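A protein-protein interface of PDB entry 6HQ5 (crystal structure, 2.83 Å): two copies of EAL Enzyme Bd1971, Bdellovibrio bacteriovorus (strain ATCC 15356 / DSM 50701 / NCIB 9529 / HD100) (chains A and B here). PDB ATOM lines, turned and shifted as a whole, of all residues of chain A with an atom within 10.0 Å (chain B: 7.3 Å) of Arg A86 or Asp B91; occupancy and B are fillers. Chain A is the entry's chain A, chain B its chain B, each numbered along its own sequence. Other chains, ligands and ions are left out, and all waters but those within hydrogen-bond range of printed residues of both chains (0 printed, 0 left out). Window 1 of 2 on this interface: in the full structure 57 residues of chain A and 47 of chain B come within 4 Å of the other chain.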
ATOM      1  N   ILE A  58      16.752  26.028  12.539  1.00  0.00           N
ATOM      2  CA  ILE A  58      16.615  25.632  11.136  1.00  0.00           C
ATOM      3  C   ILE A  58      17.762  26.141  10.263  1.00  0.00           C
ATOM      4  O   ILE A  58      18.389  25.359   9.549  1.00  0.00           O
ATOM      5  CB  ILE A  58      15.270  26.114  10.551  1.00  0.00           C
ATOM      6  CG1 ILE A  58      14.108  25.420  11.266  1.00  0.00           C
ATOM      7  CG2 ILE A  58      15.188  25.831   9.054  1.00  0.00           C
ATOM      8  CD1 ILE A  58      12.778  26.121  11.112  1.00  0.00           C
ATOM      9  N   VAL A  78      12.206  20.641  22.464  1.00  0.00           N
ATOM     10  CA  VAL A  78      12.339  20.073  21.123  1.00  0.00           C
ATOM     11  C   VAL A  78      13.753  20.331  20.631  1.00  0.00           C
ATOM     12  O   VAL A  78      14.194  21.477  20.574  1.00  0.00           O
ATOM     13  CB  VAL A  78      11.343  20.698  20.130  1.00  0.00           C
ATOM     14  CG1 VAL A  78      11.462  20.034  18.760  1.00  0.00           C
ATOM     15  CG2 VAL A  78       9.929  20.590  20.675  1.00  0.00           C
ATOM     16  N   THR A  79      14.442  19.262  20.244  1.00  0.00           N
ATOM     17  CA  THR A  79      15.879  19.314  19.994  1.00  0.00           C
ATOM     18  C   THR A  79      16.228  19.869  18.618  1.00  0.00           C
ATOM     19  O   THR A  79      15.433  19.785  17.675  1.00  0.00           O
ATOM     20  CB  THR A  79      16.507  17.909  20.116  1.00  0.00           C
ATOM     21  OG1 THR A  79      15.832  17.167  21.137  1.00  0.00           O
ATOM     22  CG2 THR A  79      17.988  18.004  20.462  1.00  0.00           C
ATOM     23  N   LYS A  80      17.428  20.447  18.527  1.00  0.00           N
ATOM     24  CA  LYS A  80      17.999  20.882  17.261  1.00  0.00           C
ATOM     25  C   LYS A  80      18.040  19.706  16.295  1.00  0.00           C
ATOM     26  O   LYS A  80      17.495  19.782  15.202  1.00  0.00           O
ATOM     27  CB  LYS A  80      19.409  21.440  17.484  1.00  0.00           C
ATOM     28  CG  LYS A  80      20.083  21.984  16.236  1.00  0.00           C
ATOM     29  CD  LYS A  80      21.356  22.741  16.577  1.00  0.00           C
ATOM     30  CE  LYS A  80      22.101  23.173  15.324  1.00  0.00           C
ATOM     31  NZ  LYS A  80      21.425  24.288  14.600  1.00  0.00           N
ATOM     32  N   GLN A  81      18.672  18.615  16.720  1.00  0.00           N
ATOM     33  CA  GLN A  81      18.756  17.388  15.926  1.00  0.00           C
ATOM     34  C   GLN A  81      17.409  17.000  15.307  1.00  0.00           C
ATOM     35  O   GLN A  81      17.354  16.615  14.142  1.00  0.00           O
ATOM     36  CB  GLN A  81      19.304  16.240  16.790  1.00  0.00           C
ATOM     37  CG  GLN A  81      19.251  14.851  16.163  1.00  0.00           C
ATOM     38  CD  GLN A  81      19.858  14.804  14.771  1.00  0.00           C
ATOM     39  OE1 GLN A  81      20.934  15.355  14.531  1.00  0.00           O
ATOM     40  NE2 GLN A  81      19.168  14.148  13.844  1.00  0.00           N
ATOM     41  N   GLN A  82      16.335  17.116  16.083  1.00  0.00           N
ATOM     42  CA  GLN A  82      15.001  16.700  15.639  1.00  0.00           C
ATOM     43  C   GLN A  82      14.430  17.542  14.506  1.00  0.00           C
ATOM     44  O   GLN A  82      13.811  17.006  13.579  1.00  0.00           O
ATOM     45  CB  GLN A  82      14.028  16.706  16.812  1.00  0.00           C
ATOM     46  CG  GLN A  82      14.287  15.620  17.821  1.00  0.00           C
ATOM     47  CD  GLN A  82      13.376  15.825  19.020  1.00  0.00           C
ATOM     48  OE1 GLN A  82      13.572  16.751  19.800  1.00  0.00           O
ATOM     49  NE2 GLN A  82      12.336  15.001  19.137  1.00  0.00           N
ATOM     50  N   VAL A  83      14.626  18.856  14.574  1.00  0.00           N
ATOM     51  CA  VAL A  83      14.079  19.732  13.538  1.00  0.00           C
ATOM     52  C   VAL A  83      14.895  19.606  12.237  1.00  0.00           C
ATOM     53  O   VAL A  83      14.323  19.477  11.152  1.00  0.00           O
ATOM     54  CB  VAL A  83      13.943  21.211  14.005  1.00  0.00           C
ATOM     55  CG1 VAL A  83      13.165  21.313  15.318  1.00  0.00           C
ATOM     56  CG2 VAL A  83      15.294  21.899  14.142  1.00  0.00           C
ATOM     57  N   LEU A  84      16.224  19.606  12.352  1.00  0.00           N
ATOM     58  CA  LEU A  84      17.109  19.460  11.186  1.00  0.00           C
ATOM     59  C   LEU A  84      16.856  18.145  10.461  1.00  0.00           C
ATOM     60  O   LEU A  84      16.780  18.119   9.238  1.00  0.00           O
ATOM     61  CB  LEU A  84      18.589  19.550  11.573  1.00  0.00           C
ATOM     62  CG  LEU A  84      19.208  20.927  11.823  1.00  0.00           C
ATOM     63  CD1 LEU A  84      18.677  21.958  10.840  1.00  0.00           C
ATOM     64  CD2 LEU A  84      18.992  21.392  13.246  1.00  0.00           C
ATOM     65  N   GLU A  85      16.730  17.066  11.230  1.00  0.00           N
ATOM     66  CA  GLU A  85      16.429  15.736  10.695  1.00  0.00           C
ATOM     67  C   GLU A  85      15.192  15.754   9.798  1.00  0.00           C
ATOM     68  O   GLU A  85      15.162  15.091   8.761  1.00  0.00           O
ATOM     69  CB  GLU A  85      16.252  14.736  11.855  1.00  0.00           C
ATOM     70  CG  GLU A  85      15.629  13.369  11.509  1.00  0.00           C
ATOM     71  CD  GLU A  85      16.192  12.224  12.344  1.00  0.00           C
ATOM     72  OE1 GLU A  85      16.688  12.478  13.467  1.00  0.00           O
ATOM     73  OE2 GLU A  85      16.132  11.060  11.874  1.00  0.00           O
ATOM     74  N   ARG A  86      14.186  16.528  10.193  1.00  0.00           N
ATOM     75  CA  ARG A  86      12.925  16.567   9.462  1.00  0.00           C
ATOM     76  C   ARG A  86      12.933  17.538   8.279  1.00  0.00           C
ATOM     77  O   ARG A  86      12.367  17.229   7.230  1.00  0.00           O
ATOM     78  CB  ARG A  86      11.780  16.869  10.430  1.00  0.00           C
ATOM     79  CG  ARG A  86      11.469  15.687  11.335  1.00  0.00           C
ATOM     80  CD  ARG A  86      10.698  16.095  12.575  1.00  0.00           C
ATOM     81  NE  ARG A  86      10.419  14.966  13.458  1.00  0.00           N
ATOM     82  CZ  ARG A  86       9.410  14.109  13.299  1.00  0.00           C
ATOM     83  NH1 ARG A  86       8.550  14.227  12.288  1.00  0.00           N
ATOM     84  NH2 ARG A  86       9.261  13.118  14.166  1.00  0.00           N
ATOM     85  N   VAL A  87      13.562  18.698   8.440  1.00  0.00           N
ATOM     86  CA  VAL A  87      13.656  19.670   7.334  1.00  0.00           C
ATOM     87  C   VAL A  87      14.624  19.223   6.232  1.00  0.00           C
ATOM     88  O   VAL A  87      14.329  19.374   5.048  1.00  0.00           O
ATOM     89  CB  VAL A  87      14.002  21.099   7.827  1.00  0.00           C
ATOM     90  CG1 VAL A  87      15.454  21.228   8.277  1.00  0.00           C
ATOM     91  CG2 VAL A  87      13.677  22.137   6.759  1.00  0.00           C
ATOM     92  N   SER A  88      15.764  18.663   6.620  1.00  0.00           N
ATOM     93  CA  SER A  88      16.764  18.204   5.647  1.00  0.00           C
ATOM     94  C   SER A  88      16.221  17.101   4.730  1.00  0.00           C
ATOM     95  O   SER A  88      16.580  17.030   3.553  1.00  0.00           O
ATOM     96  CB  SER A  88      18.011  17.690   6.362  1.00  0.00           C
ATOM     97  OG  SER A  88      17.743  16.469   7.025  1.00  0.00           O
ATOM     98  N   THR A  89      15.353  16.252   5.279  1.00  0.00           N
ATOM     99  CA  THR A  89      14.756  15.153   4.524  1.00  0.00           C
ATOM    100  C   THR A  89      13.431  15.545   3.850  1.00  0.00           C
ATOM    101  O   THR A  89      12.666  14.672   3.437  1.00  0.00           O
ATOM    102  CB  THR A  89      14.516  13.933   5.439  1.00  0.00           C
ATOM    103  OG1 THR A  89      13.591  14.279   6.478  1.00  0.00           O
ATOM    104  CG2 THR A  89      15.828  13.459   6.062  1.00  0.00           C
ATOM    105  N   ALA A  90      13.167  16.846   3.735  1.00  0.00           N
ATOM    106  CA  ALA A  90      11.938  17.347   3.120  1.00  0.00           C
ATOM    107  C   ALA A  90      12.141  17.652   1.640  1.00  0.00           C
ATOM    108  O   ALA A  90      13.269  17.703   1.154  1.00  0.00           O
ATOM    109  CB  ALA A  90      11.467  18.595   3.848  1.00  0.00           C
ATOM    110  N   ASP A  91      11.030  17.864   0.936  1.00  0.00           N
ATOM    111  CA  ASP A  91      11.043  18.179  -0.496  1.00  0.00           C
ATOM    112  C   ASP A  91      11.920  19.402  -0.778  1.00  0.00           C
ATOM    113  O   ASP A  91      12.078  20.266   0.079  1.00  0.00           O
ATOM    114  CB  ASP A  91       9.606  18.406  -0.989  1.00  0.00           C
ATOM    115  CG  ASP A  91       9.532  18.765  -2.462  1.00  0.00           C
ATOM    116  OD1 ASP A  91      10.364  18.270  -3.246  1.00  0.00           O
ATOM    117  OD2 ASP A  91       8.637  19.546  -2.839  1.00  0.00           O
ATOM    118  N   LYS A  92      12.481  19.465  -1.983  1.00  0.00           N
ATOM    119  CA  LYS A  92      13.476  20.486  -2.331  1.00  0.00           C
ATOM    120  C   LYS A  92      12.925  21.915  -2.372  1.00  0.00           C
ATOM    121  O   LYS A  92      13.588  22.841  -1.899  1.00  0.00           O
ATOM    122  CB  LYS A  92      14.136  20.148  -3.676  1.00  0.00           C
ATOM    123  CG  LYS A  92      15.022  18.912  -3.628  1.00  0.00           C
ATOM    124  CD  LYS A  92      16.342  19.162  -2.901  1.00  0.00           C
ATOM    125  CE  LYS A  92      16.454  18.299  -1.655  1.00  0.00           C
ATOM    126  NZ  LYS A  92      17.675  18.596  -0.858  1.00  0.00           N
ATOM    127  N   VAL A  94       9.947  22.822  -0.949  1.00  0.00           N
ATOM    128  CA  VAL A  94       9.444  23.018   0.411  1.00  0.00           C
ATOM    129  C   VAL A  94      10.532  23.635   1.302  1.00  0.00           C
ATOM    130  O   VAL A  94      10.241  24.489   2.134  1.00  0.00           O
ATOM    131  CB  VAL A  94       8.920  21.692   1.016  1.00  0.00           C
ATOM    132  CG1 VAL A  94       8.733  21.799   2.526  1.00  0.00           C
ATOM    133  CG2 VAL A  94       7.611  21.288   0.349  1.00  0.00           C
ATOM    134  N   GLN A  95      11.780  23.214   1.106  1.00  0.00           N
ATOM    135  CA  GLN A  95      12.910  23.774   1.849  1.00  0.00           C
ATOM    136  C   GLN A  95      13.232  25.223   1.473  1.00  0.00           C
ATOM    137  O   GLN A  95      13.702  25.988   2.317  1.00  0.00           O
ATOM    138  CB  GLN A  95      14.154  22.894   1.689  1.00  0.00           C
ATOM    139  CG  GLN A  95      14.029  21.569   2.422  1.00  0.00           C
ATOM    140  CD  GLN A  95      15.296  20.740   2.370  1.00  0.00           C
ATOM    141  OE1 GLN A  95      16.365  21.203   2.763  1.00  0.00           O
ATOM    142  NE2 GLN A  95      15.178  19.501   1.906  1.00  0.00           N
ATOM    143  N   MET A  98      10.648  27.471   3.157  1.00  0.00           N
ATOM    144  CA  MET A  98      11.066  27.670   4.550  1.00  0.00           C
ATOM    145  C   MET A  98      12.095  28.793   4.706  1.00  0.00           C
ATOM    146  O   MET A  98      11.955  29.662   5.568  1.00  0.00           O
ATOM    147  CB  MET A  98      11.633  26.372   5.124  1.00  0.00           C
ATOM    148  CG  MET A  98      10.612  25.252   5.257  1.00  0.00           C
ATOM    149  SD  MET A  98       9.632  25.332   6.764  1.00  0.00           S
ATOM    150  CE  MET A  98      10.871  24.878   7.979  1.00  0.00           C
ATOM    151  N   ARG B  86       3.135  19.406  -3.220  1.00  0.00           N
ATOM    152  CA  ARG B  86       4.402  19.226  -2.515  1.00  0.00           C
ATOM    153  C   ARG B  86       4.309  19.463  -1.009  1.00  0.00           C
ATOM    154  O   ARG B  86       4.943  18.738  -0.240  1.00  0.00           O
ATOM    155  CB  ARG B  86       5.475  20.114  -3.135  1.00  0.00           C
ATOM    156  CG  ARG B  86       5.925  19.601  -4.491  1.00  0.00           C
ATOM    157  CD  ARG B  86       6.614  20.675  -5.310  1.00  0.00           C
ATOM    158  NE  ARG B  86       7.068  20.169  -6.605  1.00  0.00           N
ATOM    159  CZ  ARG B  86       6.288  19.958  -7.667  1.00  0.00           C
ATOM    160  NH1 ARG B  86       4.981  20.194  -7.619  1.00  0.00           N
ATOM    161  NH2 ARG B  86       6.825  19.492  -8.789  1.00  0.00           N
ATOM    162  N   VAL B  87       3.533  20.463  -0.589  1.00  0.00           N
ATOM    163  CA  VAL B  87       3.361  20.739   0.844  1.00  0.00           C
ATOM    164  C   VAL B  87       2.495  19.680   1.533  1.00  0.00           C
ATOM    165  O   VAL B  87       2.814  19.256   2.647  1.00  0.00           O
ATOM    166  CB  VAL B  87       2.815  22.166   1.139  1.00  0.00           C
ATOM    167  CG1 VAL B  87       3.741  23.214   0.540  1.00  0.00           C
ATOM    168  CG2 VAL B  87       1.390  22.348   0.634  1.00  0.00           C
ATOM    169  N   SER B  88       1.422  19.242   0.871  1.00  0.00           N
ATOM    170  CA  SER B  88       0.518  18.238   1.442  1.00  0.00           C
ATOM    171  C   SER B  88       1.231  16.910   1.697  1.00  0.00           C
ATOM    172  O   SER B  88       0.927  16.212   2.666  1.00  0.00           O
ATOM    173  CB  SER B  88      -0.682  18.003   0.523  1.00  0.00           C
ATOM    174  OG  SER B  88      -0.285  17.321  -0.656  1.00  0.00           O
ATOM    175  N   THR B  89       2.183  16.573   0.830  1.00  0.00           N
ATOM    176  CA  THR B  89       2.955  15.332   0.952  1.00  0.00           C
ATOM    177  C   THR B  89       4.256  15.511   1.754  1.00  0.00           C
ATOM    178  O   THR B  89       5.148  14.663   1.687  1.00  0.00           O
ATOM    179  CB  THR B  89       3.299  14.764  -0.442  1.00  0.00           C
ATOM    180  OG1 THR B  89       4.131  15.692  -1.149  1.00  0.00           O
ATOM    181  CG2 THR B  89       2.028  14.504  -1.251  1.00  0.00           C
ATOM    182  N   ALA B  90       4.354  16.601   2.516  1.00  0.00           N
ATOM    183  CA  ALA B  90       5.532  16.878   3.338  1.00  0.00           C
ATOM    184  C   ALA B  90       5.344  16.334   4.749  1.00  0.00           C
ATOM    185  O   ALA B  90       4.231  15.983   5.150  1.00  0.00           O
ATOM    186  CB  ALA B  90       5.801  18.373   3.387  1.00  0.00           C
ATOM    187  N   ASP B  91       6.441  16.286   5.499  1.00  0.00           N
ATOM    188  CA  ASP B  91       6.432  15.796   6.877  1.00  0.00           C
ATOM    189  C   ASP B  91       5.412  16.561   7.727  1.00  0.00           C
ATOM    190  O   ASP B  91       5.112  17.727   7.448  1.00  0.00           O
ATOM    191  CB  ASP B  91       7.838  15.912   7.475  1.00  0.00           C
ATOM    192  CG  ASP B  91       7.909  15.442   8.914  1.00  0.00           C
ATOM    193  OD1 ASP B  91       7.171  14.504   9.281  1.00  0.00           O
ATOM    194  OD2 ASP B  91       8.709  16.009   9.682  1.00  0.00           O
ATOM    195  N   LYS B  92       4.883  15.903   8.759  1.00  0.00           N
ATOM    196  CA  LYS B  92       3.769  16.458   9.538  1.00  0.00           C
ATOM    197  C   LYS B  92       4.133  17.703  10.353  1.00  0.00           C
ATOM    198  O   LYS B  92       3.339  18.645  10.421  1.00  0.00           O
ATOM    199  CB  LYS B  92       3.146  15.405  10.465  1.00  0.00           C
ATOM    200  CG  LYS B  92       1.667  15.653  10.735  1.00  0.00           C
ATOM    201  CD  LYS B  92       1.108  14.733  11.801  1.00  0.00           C
ATOM    202  CE  LYS B  92      -0.101  15.358  12.478  1.00  0.00           C
ATOM    203  NZ  LYS B  92      -0.682  14.479  13.523  1.00  0.00           N
ATOM    204  N   VAL B  93       5.313  17.710  10.974  1.00  0.00           N
ATOM    205  CA  VAL B  93       5.736  18.870  11.769  1.00  0.00           C
ATOM    206  C   VAL B  93       6.242  19.976  10.849  1.00  0.00           C
ATOM    207  O   VAL B  93       6.007  21.154  11.112  1.00  0.00           O
ATOM    208  CB  VAL B  93       6.800  18.541  12.847  1.00  0.00           C
ATOM    209  CG1 VAL B  93       6.407  17.304  13.646  1.00  0.00           C
ATOM    210  CG2 VAL B  93       8.189  18.385  12.245  1.00  0.00           C
ATOM    211  N   VAL B  94       6.918  19.591   9.766  1.00  0.00           N
ATOM    212  CA  VAL B  94       7.352  20.541   8.742  1.00  0.00           C
ATOM    213  C   VAL B  94       6.170  21.395   8.275  1.00  0.00           C
ATOM    214  O   VAL B  94       6.324  22.593   8.039  1.00  0.00           O
ATOM    215  CB  VAL B  94       8.019  19.822   7.545  1.00  0.00           C
ATOM    216  CG1 VAL B  94       8.139  20.741   6.333  1.00  0.00           C
ATOM    217  CG2 VAL B  94       9.390  19.294   7.950  1.00  0.00           C
ATOM    218  N   GLN B  95       4.994  20.781   8.162  1.00  0.00           N
ATOM    219  CA  GLN B  95       3.778  21.506   7.789  1.00  0.00           C
ATOM    220  C   GLN B  95       3.287  22.470   8.881  1.00  0.00           C
ATOM    221  O   GLN B  95       2.697  23.499   8.568  1.00  0.00           O
ATOM    222  CB  GLN B  95       2.668  20.529   7.387  1.00  0.00           C
ATOM    223  CG  GLN B  95       2.939  19.821   6.066  1.00  0.00           C
ATOM    224  CD  GLN B  95       1.791  18.940   5.618  1.00  0.00           C
ATOM    225  OE1 GLN B  95       0.660  19.406   5.473  1.00  0.00           O
ATOM    226  NE2 GLN B  95       2.079  17.663   5.378  1.00  0.00           N
ATOM    227  N   LEU B  96       3.516  22.132  10.152  1.00  0.00           N
ATOM    228  CA  LEU B  96       3.260  23.069  11.265  1.00  0.00           C
ATOM    229  C   LEU B  96       4.181  24.285  11.177  1.00  0.00           C
ATOM    230  O   LEU B  96       3.715  25.433  11.142  1.00  0.00           O
ATOM    231  CB  LEU B  96       3.377  22.386  12.646  1.00  0.00           C
ATOM    232  CG  LEU B  96       2.027  21.918  13.195  1.00  0.00           C
ATOM    233  CD1 LEU B  96       1.533  20.707  12.412  1.00  0.00           C
ATOM    234  CD2 LEU B  96       2.132  21.611  14.682  1.00  0.00           C
ATOM    235  N   LEU B  97       5.484  24.020  11.111  1.00  0.00           N
ATOM    236  CA  LEU B  97       6.488  25.071  10.964  1.00  0.00           C
ATOM    237  C   LEU B  97       6.095  26.073   9.875  1.00  0.00           C
ATOM    238  O   LEU B  97       6.292  27.274  10.041  1.00  0.00           O
ATOM    239  CB  LEU B  97       7.866  24.475  10.655  1.00  0.00           C
ATOM    240  CG  LEU B  97       8.671  23.923  11.844  1.00  0.00           C
ATOM    241  CD1 LEU B  97       8.376  22.461  12.135  1.00  0.00           C
ATOM    242  CD2 LEU B  97      10.160  24.087  11.599  1.00  0.00           C
ATOM    243  N   ALA B 136       1.116  15.752  15.955  1.00  0.00           N
ATOM    244  CA  ALA B 136       2.448  16.108  15.459  1.00  0.00           C
ATOM    245  C   ALA B 136       3.389  16.435  16.614  1.00  0.00           C
ATOM    246  O   ALA B 136       4.523  15.954  16.645  1.00  0.00           O
ATOM    247  CB  ALA B 136       2.376  17.279  14.491  1.00  0.00           C
ATOM    248  N   GLN B 139       4.411  13.310  18.692  1.00  0.00           N
ATOM    249  CA  GLN B 139       5.491  12.531  18.105  1.00  0.00           C
ATOM    250  C   GLN B 139       6.860  13.001  18.600  1.00  0.00           C
ATOM    251  O   GLN B 139       7.724  12.180  18.928  1.00  0.00           O
ATOM    252  CB  GLN B 139       5.430  12.620  16.581  1.00  0.00           C
ATOM    253  CG  GLN B 139       6.423  11.728  15.857  1.00  0.00           C
ATOM    254  CD  GLN B 139       6.138  11.651  14.371  1.00  0.00           C
ATOM    255  OE1 GLN B 139       5.458  12.516  13.812  1.00  0.00           O
ATOM    256  NE2 GLN B 139       6.659  10.615  13.722  1.00  0.00           N
ATOM    257  N   ILE B 140       7.049  14.319  18.657  1.00  0.00           N
ATOM    258  CA  ILE B 140       8.312  14.900  19.128  1.00  0.00           C
ATOM    259  C   ILE B 140       8.561  14.535  20.578  1.00  0.00           C
ATOM    260  O   ILE B 140       9.661  14.099  20.938  1.00  0.00           O
ATOM    261  CB  ILE B 140       8.316  16.437  19.014  1.00  0.00           C
ATOM    262  CG1 ILE B 140       8.212  16.861  17.552  1.00  0.00           C
ATOM    263  CG2 ILE B 140       9.593  17.037  19.585  1.00  0.00           C
ATOM    264  CD1 ILE B 140       6.963  17.641  17.232  1.00  0.00           C
ATOM    265  N   GLU B 143       9.521  10.677  21.035  1.00  0.00           N
ATOM    266  CA  GLU B 143      10.921  10.372  20.688  1.00  0.00           C
ATOM    267  C   GLU B 143      11.871  10.663  21.840  1.00  0.00           C
ATOM    268  O   GLU B 143      12.762   9.860  22.144  1.00  0.00           O
ATOM    269  CB  GLU B 143      11.382  11.191  19.482  1.00  0.00           C
ATOM    270  CG  GLU B 143      10.793  10.744  18.162  1.00  0.00           C
ATOM    271  CD  GLU B 143      11.123  11.705  17.036  1.00  0.00           C
ATOM    272  OE1 GLU B 143      12.270  12.202  16.986  1.00  0.00           O
ATOM    273  OE2 GLU B 143      10.234  11.958  16.197  1.00  0.00           O
ATOM    274  N   ASN B 198      12.939   4.654  12.624  1.00  0.00           N
ATOM    275  CA  ASN B 198      12.894   5.806  11.707  1.00  0.00           C
ATOM    276  C   ASN B 198      13.403   7.092  12.358  1.00  0.00           C
ATOM    277  O   ASN B 198      12.799   8.149  12.214  1.00  0.00           O
ATOM    278  CB  ASN B 198      11.461   6.038  11.226  1.00  0.00           C
ATOM    279  CG  ASN B 198      10.866   4.823  10.554  1.00  0.00           C
ATOM    280  OD1 ASN B 198       9.827   4.326  10.979  1.00  0.00           O
ATOM    281  ND2 ASN B 198      11.523   4.330   9.508  1.00  0.00           N
ATOM    282  N   SER B 199      14.519   6.999  13.070  1.00  0.00           N
ATOM    283  CA  SER B 199      15.040   8.106  13.849  1.00  0.00           C
ATOM    284  C   SER B 199      16.547   7.909  13.960  1.00  0.00           C
ATOM    285  O   SER B 199      17.025   6.790  13.812  1.00  0.00           O
ATOM    286  CB  SER B 199      14.427   8.070  15.238  1.00  0.00           C
ATOM    287  OG  SER B 199      13.027   8.264  15.180  1.00  0.00           O
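Arg A86 touches Asp B91, and with the chains exchanged Asp A91 touches Arg B86. Arg A86 touches Val B94, and with the chains exchanged Val A94 touches Arg B86. Val B94 touches its own counterpart, Val A94. Of the 14 pairs that touch across the chains among the printed residues, 5 have their exchanged pair printed and touching as well.
Ile A58 touches Leu B97 (CD1 to CD2, 3.4 Å). Ile B140 touches Val A78 (CG2 to CG1, 3.6 Å). CA of Ser B199 touches OE2 of Glu A85 (3.7 Å). Arg A86 touches Val B93. Arg A86 touches Val B94. NH2 of Arg A86 touches CD of Gln B139 (3.5 Å). Arg B86 touches Asp A91. CG2 of Val A94 touches O of Arg B86 (3.7 Å). CG1 of Val B94 touches CG1 of Val A94, at 3.996 Å. CD2 of Leu B97 touches CE of Met A98 (3.8 Å).
The backbone carbonyl oxygen of Ile B140 is in hydrogen-bond range of the side-chain amide nitrogen of Gln A82 (3.3 Å). OD2 of Asp B91 lies within salt-bridge range of NH1 of Arg A86, at 3.2 Å. The guanidinium group (NH2) of Arg A86 is in salt-bridge range of the side-chain carboxylate (OE2) of Glu B143, at 2.5 Å.
Of chain A, only Arg A86 comes within 4 Å of Asp B91. Lys B92 touches none of the printed residues of chain A. Val B93 touches just one residue of chain A: Arg A86 (3.4 Å). Gln B95 touches none of the printed residues of chain A. Printed residues of chain A within 4 Å of Ile B140: Val A78 (3.6 Å) and Gln A82 (3.3 Å). Of the printed residues of chain A, Ser B199 touches Glu A85. The nearest residue of chain A that does not touch Asp B91 is Val A87 (5.7 Å).
OE1 of Gln A82 lies within hydrogen-bond range of OG1 of Thr A79 (2.7 Å). The side-chain amide nitrogen (NE2) of Gln A81 lies within hydrogen-bond range of the side-chain carboxylate (OE1) of Glu A85, 3.0 Å away. O of Glu A85 is in hydrogen-bond range of OG of Ser A88, at 3.4 Å. O of Glu A85 lies within hydrogen-bond range of OG1 of Thr A89. The backbone carbonyl oxygen (O) of Arg A86 is in hydrogen-bond range of the side-chain hydroxyl (OG1) of Thr A89 (3.3 Å). The backbone carbonyl oxygen of Arg B86 lies within hydrogen-bond range of the side-chain hydroxyl of Thr B89.
Hydrophobic or aromatic side chains of chain A within 4 Å of the printed part of chain B: Ile A58, Val A78, Val A94 and Met A98. Among the printed residues, Asp or Glu carboxylates within 4 Å of a Lys or Arg side-chain nitrogen of the other chain: Arg A86 with Asp B91 (3.2 Å) and Arg A86 with Glu B143 (2.5 Å).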
